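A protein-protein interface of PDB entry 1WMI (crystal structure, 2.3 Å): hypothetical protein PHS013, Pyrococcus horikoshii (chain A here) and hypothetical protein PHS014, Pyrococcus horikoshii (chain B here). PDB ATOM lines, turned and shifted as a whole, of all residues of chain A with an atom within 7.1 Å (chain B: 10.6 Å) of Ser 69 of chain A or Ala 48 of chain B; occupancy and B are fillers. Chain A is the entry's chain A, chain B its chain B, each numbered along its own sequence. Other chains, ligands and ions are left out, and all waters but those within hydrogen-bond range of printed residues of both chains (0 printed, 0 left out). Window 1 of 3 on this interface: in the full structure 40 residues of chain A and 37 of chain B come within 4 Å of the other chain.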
ATOM      1  N   ARG A   4     -32.018 -18.375 -16.699  1.00  0.00           N
ATOM      2  CA  ARG A   4     -31.123 -17.763 -15.733  1.00  0.00           C
ATOM      3  C   ARG A   4     -30.962 -16.306 -16.174  1.00  0.00           C
ATOM      4  O   ARG A   4     -30.624 -16.034 -17.333  1.00  0.00           O
ATOM      5  CB  ARG A   4     -29.780 -18.488 -15.740  1.00  0.00           C
ATOM      6  CG  ARG A   4     -28.971 -18.329 -14.467  1.00  0.00           C
ATOM      7  CD  ARG A   4     -28.015 -19.512 -14.296  1.00  0.00           C
ATOM      8  NE  ARG A   4     -27.302 -19.504 -13.018  1.00  0.00           N
ATOM      9  CZ  ARG A   4     -26.251 -18.736 -12.749  1.00  0.00           C
ATOM     10  NH1 ARG A   4     -25.670 -18.801 -11.555  1.00  0.00           N
ATOM     11  NH2 ARG A   4     -25.773 -17.910 -13.673  1.00  0.00           N
ATOM     12  N   PRO A  37     -39.314 -15.266 -21.460  1.00  0.00           N
ATOM     13  CA  PRO A  37     -38.249 -14.416 -22.008  1.00  0.00           C
ATOM     14  C   PRO A  37     -38.726 -13.154 -22.740  1.00  0.00           C
ATOM     15  O   PRO A  37     -38.032 -12.134 -22.757  1.00  0.00           O
ATOM     16  CB  PRO A  37     -37.494 -15.374 -22.921  1.00  0.00           C
ATOM     17  CG  PRO A  37     -38.584 -16.282 -23.405  1.00  0.00           C
ATOM     18  CD  PRO A  37     -39.320 -16.581 -22.120  1.00  0.00           C
ATOM     19  N   LEU A  54     -28.955 -15.504 -30.298  1.00  0.00           N
ATOM     20  CA  LEU A  54     -29.286 -14.549 -29.264  1.00  0.00           C
ATOM     21  C   LEU A  54     -30.103 -13.451 -29.922  1.00  0.00           C
ATOM     22  O   LEU A  54     -29.854 -13.061 -31.068  1.00  0.00           O
ATOM     23  CB  LEU A  54     -28.032 -13.951 -28.608  1.00  0.00           C
ATOM     24  CG  LEU A  54     -26.817 -13.487 -29.415  1.00  0.00           C
ATOM     25  CD1 LEU A  54     -27.230 -12.621 -30.586  1.00  0.00           C
ATOM     26  CD2 LEU A  54     -25.887 -12.723 -28.482  1.00  0.00           C
ATOM     27  N   ASP A  55     -31.113 -12.986 -29.206  1.00  0.00           N
ATOM     28  CA  ASP A  55     -31.962 -11.918 -29.694  1.00  0.00           C
ATOM     29  C   ASP A  55     -31.785 -10.761 -28.735  1.00  0.00           C
ATOM     30  O   ASP A  55     -31.523 -10.971 -27.548  1.00  0.00           O
ATOM     31  CB  ASP A  55     -33.429 -12.347 -29.684  1.00  0.00           C
ATOM     32  CG  ASP A  55     -33.727 -13.425 -30.686  1.00  0.00           C
ATOM     33  OD1 ASP A  55     -34.842 -13.980 -30.639  1.00  0.00           O
ATOM     34  OD2 ASP A  55     -32.852 -13.708 -31.525  1.00  0.00           O
ATOM     35  N   LEU A  56     -31.905  -9.544 -29.257  1.00  0.00           N
ATOM     36  CA  LEU A  56     -31.816  -8.346 -28.436  1.00  0.00           C
ATOM     37  C   LEU A  56     -33.259  -7.872 -28.343  1.00  0.00           C
ATOM     38  O   LEU A  56     -34.022  -8.005 -29.298  1.00  0.00           O
ATOM     39  CB  LEU A  56     -30.947  -7.276 -29.097  1.00  0.00           C
ATOM     40  CG  LEU A  56     -29.434  -7.489 -29.109  1.00  0.00           C
ATOM     41  CD1 LEU A  56     -28.794  -6.425 -29.959  1.00  0.00           C
ATOM     42  CD2 LEU A  56     -28.881  -7.433 -27.697  1.00  0.00           C
ATOM     43  N   TYR A  57     -33.632  -7.349 -27.184  1.00  0.00           N
ATOM     44  CA  TYR A  57     -34.985  -6.873 -26.961  1.00  0.00           C
ATOM     45  C   TYR A  57     -34.963  -5.566 -26.181  1.00  0.00           C
ATOM     46  O   TYR A  57     -33.950  -5.204 -25.585  1.00  0.00           O
ATOM     47  CB  TYR A  57     -35.773  -7.919 -26.160  1.00  0.00           C
ATOM     48  CG  TYR A  57     -36.025  -9.221 -26.893  1.00  0.00           C
ATOM     49  CD1 TYR A  57     -37.057  -9.328 -27.823  1.00  0.00           C
ATOM     50  CD2 TYR A  57     -35.222 -10.342 -26.666  1.00  0.00           C
ATOM     51  CE1 TYR A  57     -37.287 -10.511 -28.501  1.00  0.00           C
ATOM     52  CE2 TYR A  57     -35.447 -11.533 -27.345  1.00  0.00           C
ATOM     53  CZ  TYR A  57     -36.485 -11.606 -28.261  1.00  0.00           C
ATOM     54  OH  TYR A  57     -36.738 -12.775 -28.929  1.00  0.00           O
ATOM     55  N   ILE A  67     -32.816  -2.880 -22.058  1.00  0.00           N
ATOM     56  CA  ILE A  67     -32.453  -3.674 -23.226  1.00  0.00           C
ATOM     57  C   ILE A  67     -31.736  -4.931 -22.747  1.00  0.00           C
ATOM     58  O   ILE A  67     -30.832  -4.865 -21.914  1.00  0.00           O
ATOM     59  CB  ILE A  67     -31.534  -2.892 -24.188  1.00  0.00           C
ATOM     60  CG1 ILE A  67     -32.249  -1.633 -24.676  1.00  0.00           C
ATOM     61  CG2 ILE A  67     -31.180  -3.761 -25.386  1.00  0.00           C
ATOM     62  CD1 ILE A  67     -31.513  -0.898 -25.801  1.00  0.00           C
ATOM     63  N   TYR A  68     -32.143  -6.079 -23.275  1.00  0.00           N
ATOM     64  CA  TYR A  68     -31.563  -7.344 -22.854  1.00  0.00           C
ATOM     65  C   TYR A  68     -31.447  -8.343 -23.985  1.00  0.00           C
ATOM     66  O   TYR A  68     -32.033  -8.162 -25.050  1.00  0.00           O
ATOM     67  CB  TYR A  68     -32.406  -7.947 -21.722  1.00  0.00           C
ATOM     68  CG  TYR A  68     -33.816  -8.357 -22.111  1.00  0.00           C
ATOM     69  CD1 TYR A  68     -34.105  -9.665 -22.481  1.00  0.00           C
ATOM     70  CD2 TYR A  68     -34.867  -7.441 -22.058  1.00  0.00           C
ATOM     71  CE1 TYR A  68     -35.408 -10.061 -22.784  1.00  0.00           C
ATOM     72  CE2 TYR A  68     -36.171  -7.824 -22.358  1.00  0.00           C
ATOM     73  CZ  TYR A  68     -36.435  -9.138 -22.717  1.00  0.00           C
ATOM     74  OH  TYR A  68     -37.723  -9.530 -22.995  1.00  0.00           O
ATOM     75  N   SER A  69     -30.678  -9.398 -23.748  1.00  0.00           N
ATOM     76  CA  SER A  69     -30.500 -10.434 -24.746  1.00  0.00           C
ATOM     77  C   SER A  69     -31.032 -11.762 -24.241  1.00  0.00           C
ATOM     78  O   SER A  69     -31.100 -12.002 -23.037  1.00  0.00           O
ATOM     79  CB  SER A  69     -29.025 -10.579 -25.098  1.00  0.00           C
ATOM     80  OG  SER A  69     -28.258 -10.838 -23.940  1.00  0.00           O
ATOM     81  N   VAL A  70     -31.420 -12.621 -25.175  1.00  0.00           N
ATOM     82  CA  VAL A  70     -31.928 -13.937 -24.832  1.00  0.00           C
ATOM     83  C   VAL A  70     -31.123 -14.956 -25.613  1.00  0.00           C
ATOM     84  O   VAL A  70     -31.096 -14.935 -26.846  1.00  0.00           O
ATOM     85  CB  VAL A  70     -33.432 -14.101 -25.191  1.00  0.00           C
ATOM     86  CG1 VAL A  70     -33.897 -15.530 -24.880  1.00  0.00           C
ATOM     87  CG2 VAL A  70     -34.264 -13.108 -24.413  1.00  0.00           C
ATOM     88  N   ASN A  71     -30.440 -15.825 -24.880  1.00  0.00           N
ATOM     89  CA  ASN A  71     -29.639 -16.882 -25.473  1.00  0.00           C
ATOM     90  C   ASN A  71     -30.509 -18.107 -25.277  1.00  0.00           C
ATOM     91  O   ASN A  71     -30.551 -18.682 -24.188  1.00  0.00           O
ATOM     92  CB  ASN A  71     -28.329 -17.040 -24.708  1.00  0.00           C
ATOM     93  CG  ASN A  71     -27.332 -17.918 -25.430  1.00  0.00           C
ATOM     94  OD1 ASN A  71     -27.651 -18.535 -26.441  1.00  0.00           O
ATOM     95  ND2 ASN A  71     -26.115 -17.983 -24.905  1.00  0.00           N
ATOM     96  N   TRP A  72     -31.223 -18.490 -26.330  1.00  0.00           N
ATOM     97  CA  TRP A  72     -32.121 -19.627 -26.261  1.00  0.00           C
ATOM     98  C   TRP A  72     -31.431 -20.954 -26.012  1.00  0.00           C
ATOM     99  O   TRP A  72     -31.970 -21.803 -25.312  1.00  0.00           O
ATOM    100  CB  TRP A  72     -32.955 -19.712 -27.538  1.00  0.00           C
ATOM    101  CG  TRP A  72     -33.719 -18.454 -27.813  1.00  0.00           C
ATOM    102  CD1 TRP A  72     -33.329 -17.420 -28.611  1.00  0.00           C
ATOM    103  CD2 TRP A  72     -34.996 -18.086 -27.272  1.00  0.00           C
ATOM    104  NE1 TRP A  72     -34.283 -16.431 -28.606  1.00  0.00           N
ATOM    105  CE2 TRP A  72     -35.318 -16.811 -27.794  1.00  0.00           C
ATOM    106  CE3 TRP A  72     -35.900 -18.705 -26.398  1.00  0.00           C
ATOM    107  CZ2 TRP A  72     -36.509 -16.143 -27.471  1.00  0.00           C
ATOM    108  CZ3 TRP A  72     -37.082 -18.044 -26.076  1.00  0.00           C
ATOM    109  CH2 TRP A  72     -37.377 -16.773 -26.613  1.00  0.00           C
ATOM    110  N   VAL A  76     -30.116 -18.179 -21.227  1.00  0.00           N
ATOM    111  CA  VAL A  76     -29.550 -17.095 -20.442  1.00  0.00           C
ATOM    112  C   VAL A  76     -30.068 -15.758 -20.938  1.00  0.00           C
ATOM    113  O   VAL A  76     -29.985 -15.452 -22.131  1.00  0.00           O
ATOM    114  CB  VAL A  76     -28.007 -17.096 -20.526  1.00  0.00           C
ATOM    115  CG1 VAL A  76     -27.442 -15.836 -19.912  1.00  0.00           C
ATOM    116  CG2 VAL A  76     -27.463 -18.301 -19.806  1.00  0.00           C
ATOM    117  N   ILE A  77     -30.622 -14.978 -20.015  1.00  0.00           N
ATOM    118  CA  ILE A  77     -31.152 -13.657 -20.320  1.00  0.00           C
ATOM    119  C   ILE A  77     -30.213 -12.658 -19.663  1.00  0.00           C
ATOM    120  O   ILE A  77     -29.920 -12.754 -18.471  1.00  0.00           O
ATOM    121  CB  ILE A  77     -32.576 -13.474 -19.752  1.00  0.00           C
ATOM    122  CG1 ILE A  77     -33.528 -14.466 -20.432  1.00  0.00           C
ATOM    123  CG2 ILE A  77     -33.049 -12.039 -19.965  1.00  0.00           C
ATOM    124  CD1 ILE A  77     -34.978 -14.275 -20.062  1.00  0.00           C
ATOM    125  N   LYS A  78     -29.722 -11.702 -20.436  1.00  0.00           N
ATOM    126  CA  LYS A  78     -28.802 -10.732 -19.873  1.00  0.00           C
ATOM    127  C   LYS A  78     -29.380  -9.353 -20.008  1.00  0.00           C
ATOM    128  O   LYS A  78     -29.830  -8.972 -21.085  1.00  0.00           O
ATOM    129  CB  LYS A  78     -27.448 -10.780 -20.587  1.00  0.00           C
ATOM    130  CG  LYS A  78     -26.739 -12.123 -20.525  1.00  0.00           C
ATOM    131  CD  LYS A  78     -25.383 -12.060 -21.215  1.00  0.00           C
ATOM    132  CE  LYS A  78     -24.762 -13.432 -21.338  1.00  0.00           C
ATOM    133  NZ  LYS A  78     -23.422 -13.348 -21.971  1.00  0.00           N
ATOM    134  N   ILE A  79     -29.386  -8.621 -18.898  1.00  0.00           N
ATOM    135  CA  ILE A  79     -29.872  -7.254 -18.888  1.00  0.00           C
ATOM    136  C   ILE A  79     -28.651  -6.447 -19.315  1.00  0.00           C
ATOM    137  O   ILE A  79     -27.699  -6.304 -18.554  1.00  0.00           O
ATOM    138  CB  ILE A  79     -30.314  -6.817 -17.469  1.00  0.00           C
ATOM    139  CG1 ILE A  79     -31.338  -7.813 -16.904  1.00  0.00           C
ATOM    140  CG2 ILE A  79     -30.872  -5.394 -17.506  1.00  0.00           C
ATOM    141  CD1 ILE A  79     -32.624  -7.918 -17.688  1.00  0.00           C
ATOM    142  N   LEU A  80     -28.673  -5.945 -20.542  1.00  0.00           N
ATOM    143  CA  LEU A  80     -27.555  -5.177 -21.071  1.00  0.00           C
ATOM    144  C   LEU A  80     -27.460  -3.733 -20.582  1.00  0.00           C
ATOM    145  O   LEU A  80     -26.410  -3.321 -20.089  1.00  0.00           O
ATOM    146  CB  LEU A  80     -27.573  -5.210 -22.601  1.00  0.00           C
ATOM    147  CG  LEU A  80     -27.225  -6.561 -23.243  1.00  0.00           C
ATOM    148  CD1 LEU A  80     -26.010  -7.176 -22.548  1.00  0.00           C
ATOM    149  CD2 LEU A  80     -28.392  -7.498 -23.127  1.00  0.00           C
ATOM    150  N   ALA B  25     -40.994 -15.809 -30.765  1.00  0.00           N
ATOM    151  CA  ALA B  25     -40.064 -14.691 -30.819  1.00  0.00           C
ATOM    152  C   ALA B  25     -39.721 -14.511 -32.297  1.00  0.00           C
ATOM    153  O   ALA B  25     -39.779 -13.409 -32.838  1.00  0.00           O
ATOM    154  CB  ALA B  25     -38.815 -15.010 -30.020  1.00  0.00           C
ATOM    155  N   GLU B  40     -25.225   0.966 -31.784  1.00  0.00           N
ATOM    156  CA  GLU B  40     -25.483   0.556 -30.426  1.00  0.00           C
ATOM    157  C   GLU B  40     -25.968  -0.880 -30.357  1.00  0.00           C
ATOM    158  O   GLU B  40     -25.672  -1.587 -29.398  1.00  0.00           O
ATOM    159  CB  GLU B  40     -26.497   1.525 -29.831  1.00  0.00           C
ATOM    160  CG  GLU B  40     -27.184   1.076 -28.573  1.00  0.00           C
ATOM    161  CD  GLU B  40     -28.137   2.133 -28.046  1.00  0.00           C
ATOM    162  OE1 GLU B  40     -28.909   2.689 -28.856  1.00  0.00           O
ATOM    163  OE2 GLU B  40     -28.125   2.404 -26.828  1.00  0.00           O
ATOM    164  N   ILE B  41     -26.697  -1.312 -31.381  1.00  0.00           N
ATOM    165  CA  ILE B  41     -27.195  -2.676 -31.431  1.00  0.00           C
ATOM    166  C   ILE B  41     -26.018  -3.612 -31.645  1.00  0.00           C
ATOM    167  O   ILE B  41     -25.974  -4.709 -31.086  1.00  0.00           O
ATOM    168  CB  ILE B  41     -28.222  -2.852 -32.564  1.00  0.00           C
ATOM    169  CG1 ILE B  41     -29.594  -2.368 -32.084  1.00  0.00           C
ATOM    170  CG2 ILE B  41     -28.279  -4.302 -33.004  1.00  0.00           C
ATOM    171  CD1 ILE B  41     -30.711  -2.600 -33.069  1.00  0.00           C
ATOM    172  N   ALA B  42     -25.065  -3.168 -32.457  1.00  0.00           N
ATOM    173  CA  ALA B  42     -23.872  -3.957 -32.722  1.00  0.00           C
ATOM    174  C   ALA B  42     -23.142  -4.127 -31.397  1.00  0.00           C
ATOM    175  O   ALA B  42     -22.791  -5.238 -31.011  1.00  0.00           O
ATOM    176  CB  ALA B  42     -22.975  -3.245 -33.730  1.00  0.00           C
ATOM    177  N   GLU B  43     -22.920  -3.014 -30.703  1.00  0.00           N
ATOM    178  CA  GLU B  43     -22.238  -3.051 -29.419  1.00  0.00           C
ATOM    179  C   GLU B  43     -23.002  -3.959 -28.466  1.00  0.00           C
ATOM    180  O   GLU B  43     -22.402  -4.672 -27.670  1.00  0.00           O
ATOM    181  CB  GLU B  43     -22.135  -1.644 -28.816  1.00  0.00           C
ATOM    182  CG  GLU B  43     -21.249  -1.568 -27.561  1.00  0.00           C
ATOM    183  CD  GLU B  43     -22.016  -1.203 -26.288  1.00  0.00           C
ATOM    184  OE1 GLU B  43     -22.539  -0.070 -26.202  1.00  0.00           O
ATOM    185  OE2 GLU B  43     -22.094  -2.048 -25.369  1.00  0.00           O
ATOM    186  N   LEU B  44     -24.330  -3.935 -28.559  1.00  0.00           N
ATOM    187  CA  LEU B  44     -25.170  -4.758 -27.691  1.00  0.00           C
ATOM    188  C   LEU B  44     -24.989  -6.249 -27.951  1.00  0.00           C
ATOM    189  O   LEU B  44     -24.864  -7.029 -27.007  1.00  0.00           O
ATOM    190  CB  LEU B  44     -26.643  -4.367 -27.846  1.00  0.00           C
ATOM    191  CG  LEU B  44     -27.010  -2.978 -27.309  1.00  0.00           C
ATOM    192  CD1 LEU B  44     -28.470  -2.700 -27.598  1.00  0.00           C
ATOM    193  CD2 LEU B  44     -26.722  -2.892 -25.813  1.00  0.00           C
ATOM    194  N   LEU B  45     -24.988  -6.653 -29.218  1.00  0.00           N
ATOM    195  CA  LEU B  45     -24.772  -8.061 -29.526  1.00  0.00           C
ATOM    196  C   LEU B  45     -23.414  -8.400 -28.934  1.00  0.00           C
ATOM    197  O   LEU B  45     -23.243  -9.426 -28.282  1.00  0.00           O
ATOM    198  CB  LEU B  45     -24.732  -8.313 -31.038  1.00  0.00           C
ATOM    199  CG  LEU B  45     -26.011  -8.630 -31.822  1.00  0.00           C
ATOM    200  CD1 LEU B  45     -26.950  -9.436 -30.941  1.00  0.00           C
ATOM    201  CD2 LEU B  45     -26.690  -7.354 -32.287  1.00  0.00           C
ATOM    202  N   GLU B  46     -22.452  -7.512 -29.166  1.00  0.00           N
ATOM    203  CA  GLU B  46     -21.093  -7.676 -28.666  1.00  0.00           C
ATOM    204  C   GLU B  46     -21.094  -7.929 -27.164  1.00  0.00           C
ATOM    205  O   GLU B  46     -20.442  -8.853 -26.677  1.00  0.00           O
ATOM    206  CB  GLU B  46     -20.271  -6.420 -28.971  1.00  0.00           C
ATOM    207  CG  GLU B  46     -18.914  -6.384 -28.292  1.00  0.00           C
ATOM    208  CD  GLU B  46     -18.203  -5.053 -28.474  1.00  0.00           C
ATOM    209  OE1 GLU B  46     -17.793  -4.733 -29.612  1.00  0.00           O
ATOM    210  OE2 GLU B  46     -18.059  -4.321 -27.472  1.00  0.00           O
ATOM    211  N   LEU B  47     -21.826  -7.102 -26.429  1.00  0.00           N
ATOM    212  CA  LEU B  47     -21.895  -7.255 -24.988  1.00  0.00           C
ATOM    213  C   LEU B  47     -22.571  -8.578 -24.628  1.00  0.00           C
ATOM    214  O   LEU B  47     -22.062  -9.348 -23.816  1.00  0.00           O
ATOM    215  CB  LEU B  47     -22.681  -6.096 -24.368  1.00  0.00           C
ATOM    216  CG  LEU B  47     -22.022  -5.273 -23.256  1.00  0.00           C
ATOM    217  CD1 LEU B  47     -23.065  -4.984 -22.187  1.00  0.00           C
ATOM    218  CD2 LEU B  47     -20.840  -6.012 -22.653  1.00  0.00           C
ATOM    219  N   ALA B  48     -23.722  -8.821 -25.246  1.00  0.00           N
ATOM    220  CA  ALA B  48     -24.500 -10.024 -25.013  1.00  0.00           C
ATOM    221  C   ALA B  48     -23.643 -11.273 -25.106  1.00  0.00           C
ATOM    222  O   ALA B  48     -23.848 -12.229 -24.359  1.00  0.00           O
ATOM    223  CB  ALA B  48     -25.647 -10.102 -26.016  1.00  0.00           C
ATOM    224  N   ARG B  49     -22.680 -11.266 -26.021  1.00  0.00           N
ATOM    225  CA  ARG B  49     -21.813 -12.421 -26.199  1.00  0.00           C
ATOM    226  C   ARG B  49     -20.558 -12.399 -25.337  1.00  0.00           C
ATOM    227  O   ARG B  49     -19.785 -13.359 -25.331  1.00  0.00           O
ATOM    228  CB  ARG B  49     -21.462 -12.591 -27.683  1.00  0.00           C
ATOM    229  CG  ARG B  49     -22.613 -13.203 -28.468  1.00  0.00           C
ATOM    230  CD  ARG B  49     -22.309 -13.396 -29.936  1.00  0.00           C
ATOM    231  NE  ARG B  49     -22.216 -12.127 -30.646  1.00  0.00           N
ATOM    232  CZ  ARG B  49     -22.716 -11.918 -31.859  1.00  0.00           C
ATOM    233  NH1 ARG B  49     -22.583 -10.731 -32.437  1.00  0.00           N
ATOM    234  NH2 ARG B  49     -23.361 -12.892 -32.491  1.00  0.00           N
ATOM    235  N   ASP B  50     -20.358 -11.308 -24.606  1.00  0.00           N
ATOM    236  CA  ASP B  50     -19.217 -11.202 -23.700  1.00  0.00           C
ATOM    237  C   ASP B  50     -19.512 -12.176 -22.567  1.00  0.00           C
ATOM    238  O   ASP B  50     -20.580 -12.113 -21.961  1.00  0.00           O
ATOM    239  CB  ASP B  50     -19.103  -9.783 -23.135  1.00  0.00           C
ATOM    240  CG  ASP B  50     -18.266  -9.720 -21.861  1.00  0.00           C
ATOM    241  OD1 ASP B  50     -18.579 -10.442 -20.891  1.00  0.00           O
ATOM    242  OD2 ASP B  50     -17.299  -8.933 -21.823  1.00  0.00           O
ATOM    243  N   GLU B  51     -18.570 -13.066 -22.275  1.00  0.00           N
ATOM    244  CA  GLU B  51     -18.775 -14.043 -21.213  1.00  0.00           C
ATOM    245  C   GLU B  51     -17.875 -13.807 -19.995  1.00  0.00           C
ATOM    246  O   GLU B  51     -17.833 -14.629 -19.078  1.00  0.00           O
ATOM    247  CB  GLU B  51     -18.558 -15.455 -21.767  1.00  0.00           C
ATOM    248  CG  GLU B  51     -19.612 -16.475 -21.349  1.00  0.00           C
ATOM    249  CD  GLU B  51     -21.012 -16.135 -21.848  1.00  0.00           C
ATOM    250  OE1 GLU B  51     -21.164 -15.837 -23.053  1.00  0.00           O
ATOM    251  OE2 GLU B  51     -21.963 -16.178 -21.036  1.00  0.00           O
ATOM    252  N   ASP B  52     -17.164 -12.684 -19.979  1.00  0.00           N
ATOM    253  CA  ASP B  52     -16.282 -12.374 -18.857  1.00  0.00           C
ATOM    254  C   ASP B  52     -17.097 -12.041 -17.607  1.00  0.00           C
ATOM    255  O   ASP B  52     -17.802 -11.037 -17.569  1.00  0.00           O
ATOM    256  CB  ASP B  52     -15.365 -11.202 -19.203  1.00  0.00           C
ATOM    257  CG  ASP B  52     -14.363 -10.895 -18.096  1.00  0.00           C
ATOM    258  OD1 ASP B  52     -13.554  -9.960 -18.281  1.00  0.00           O
ATOM    259  OD2 ASP B  52     -14.378 -11.579 -17.047  1.00  0.00           O
ATOM    260  N   PRO B  53     -16.989 -12.884 -16.565  1.00  0.00           N
ATOM    261  CA  PRO B  53     -17.670 -12.782 -15.269  1.00  0.00           C
ATOM    262  C   PRO B  53     -17.694 -11.408 -14.607  1.00  0.00           C
ATOM    263  O   PRO B  53     -18.743 -10.950 -14.156  1.00  0.00           O
ATOM    264  CB  PRO B  53     -16.931 -13.807 -14.414  1.00  0.00           C
ATOM    265  CG  PRO B  53     -16.580 -14.857 -15.405  1.00  0.00           C
ATOM    266  CD  PRO B  53     -16.085 -14.047 -16.578  1.00  0.00           C
ATOM    267  N   ASN B  55     -18.045  -8.672 -15.556  1.00  0.00           N
ATOM    268  CA  ASN B  55     -19.105  -7.831 -16.096  1.00  0.00           C
ATOM    269  C   ASN B  55     -20.525  -8.199 -15.674  1.00  0.00           C
ATOM    270  O   ASN B  55     -21.450  -7.395 -15.825  1.00  0.00           O
ATOM    271  CB  ASN B  55     -19.037  -7.842 -17.624  1.00  0.00           C
ATOM    272  CG  ASN B  55     -18.070  -6.816 -18.175  1.00  0.00           C
ATOM    273  OD1 ASN B  55     -17.778  -6.815 -19.368  1.00  0.00           O
ATOM    274  ND2 ASN B  55     -17.577  -5.929 -17.314  1.00  0.00           N
ATOM    275  N   TRP B  56     -20.700  -9.402 -15.136  1.00  0.00           N
ATOM    276  CA  TRP B  56     -22.034  -9.848 -14.763  1.00  0.00           C
ATOM    277  C   TRP B  56     -22.279 -10.313 -13.342  1.00  0.00           C
ATOM    278  O   TRP B  56     -21.367 -10.688 -12.615  1.00  0.00           O
ATOM    279  CB  TRP B  56     -22.474 -10.993 -15.682  1.00  0.00           C
ATOM    280  CG  TRP B  56     -22.138 -10.807 -17.120  1.00  0.00           C
ATOM    281  CD1 TRP B  56     -21.061 -11.313 -17.783  1.00  0.00           C
ATOM    282  CD2 TRP B  56     -22.883 -10.054 -18.075  1.00  0.00           C
ATOM    283  NE1 TRP B  56     -21.090 -10.923 -19.101  1.00  0.00           N
ATOM    284  CE2 TRP B  56     -22.199 -10.150 -19.307  1.00  0.00           C
ATOM    285  CE3 TRP B  56     -24.067  -9.311 -18.014  1.00  0.00           C
ATOM    286  CZ2 TRP B  56     -22.660  -9.521 -20.467  1.00  0.00           C
ATOM    287  CZ3 TRP B  56     -24.524  -8.688 -19.168  1.00  0.00           C
ATOM    288  CH2 TRP B  56     -23.822  -8.801 -20.376  1.00  0.00           C
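Of the 17 printed residues of chain B, 10 touch a printed residue of chain A. Of the 17 printed residues of chain A, 8 touch a printed residue of chain B. Printed residues of chain A that touch a printed residue of chain B: Leu 54, Leu 56, Tyr 57, Ile 67, Ser 69, Trp 72, Lys 78 and Leu 80. Hydrophobic or aromatic side chains of chain A that line the printed part of chain B: Leu 54, Leu 56, Tyr 57, Ile 67, Trp 72 and Leu 80. Among the printed residues, Asp or Glu carboxylates within 4 Å of a Lys or Arg side-chain nitrogen of the other chain: Lys 78 of chain A with Glu 51 of chain B.
Ala 48 of chain B touches Leu 54 of chain A (CB to CD2, 3.6 Å). Arg 49 of chain B touches Leu 54 of chain A. Ile 41 of chain B touches Leu 56 of chain A (O to CD1, 3.5 Å). CD2 of Leu 45 of chain B touches CD1 of Leu 56 of chain A, 3.3 Å away. OH of Tyr 57 of chain A touches CB of Ala 25 of chain B (3.2 Å). Leu 44 of chain B touches Ile 67 of chain A. Trp 72 of chain A touches Ala 25 of chain B (CZ2 to CB, 3.6 Å). CD1 of Leu 80 of chain A touches CD1 of Leu 47 of chain B, at 3.7 Å. Leu 80 of chain A touches Ala 48 of chain B. Leu 80 of chain A touches Trp 56 of chain B.
Ser 69 of chain A touches just one residue of chain B: Ala 48 (3.4 Å). Of the printed residues of chain A, Ala 48 of chain B touches Leu 54 (3.6 Å), Ser 69 (3.4 Å), Lys 78 (2.7 Å) and Leu 80 (3.9 Å). No residue of chain B comes within 4 Å of Val 70 of chain A. No residue of chain B comes within 4 Å of Ile 77 of chain A. Lys 78 of chain A touches just these residues of chain B: Ala 48, Asp 50, Glu 51 and Trp 56. Of the printed residues of chain A, Asp 50 of chain B touches Lys 78 (3.1 Å). Of the printed residues of chain A, Leu 47 of chain B touches Leu 80. Printed residues of chain A within 4 Å of Ala 25 of chain B: Tyr 57 (3.2 Å) and Trp 72 (3.6 Å). The nearest residue of chain A that does not touch Ala 48 of chain B is Leu 56 of chain A (4.5 Å). The nearest printed residue of chain B that does not touch Tyr 57 of chain A is Leu 44 of chain B (6.4 Å).
O of Ala 48 of chain B is in hydrogen-bond range of NZ of Lys 78 of chain A. The backbone carbonyl oxygen (O) of Asp 50 of chain B lies within hydrogen-bond range of the side-chain amino group (NZ) of Lys 78 of chain A, 3.1 Å away. The side-chain amino group of Lys 78 of chain A is in salt-bridge range of the side-chain carboxylate of Glu 51 of chain B, 3.3 Å away.
OD1 of Asp 55 of chain A is in hydrogen-bond range of NE1 of Trp 72 of chain A (3.2 Å). N of Tyr 57 of chain A lies within hydrogen-bond range of O of Tyr 68 of chain A (2.8 Å). The side-chain hydroxyl (OH) of Tyr 57 of chain A is in hydrogen-bond range of the side-chain carboxylate (OD1) of Asp 55 of chain A (2.8 Å). The side-chain amide oxygen (OD1) of Asn 55 of chain B lies close to the side-chain carboxylate (OD2) of Asp 50 of chain B (3.3 Å). The backbone carbonyl oxygen of Lys 78 of chain A sits at hydrogen-bond distance from the backbone NH of Ser 69 of chain A, 2.8 Å away. The indole nitrogen (NE1) of Trp 56 of chain B lies within hydrogen-bond range of the side-chain carboxylate (OD1) of Asp 50 of chain B (3.1 Å).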
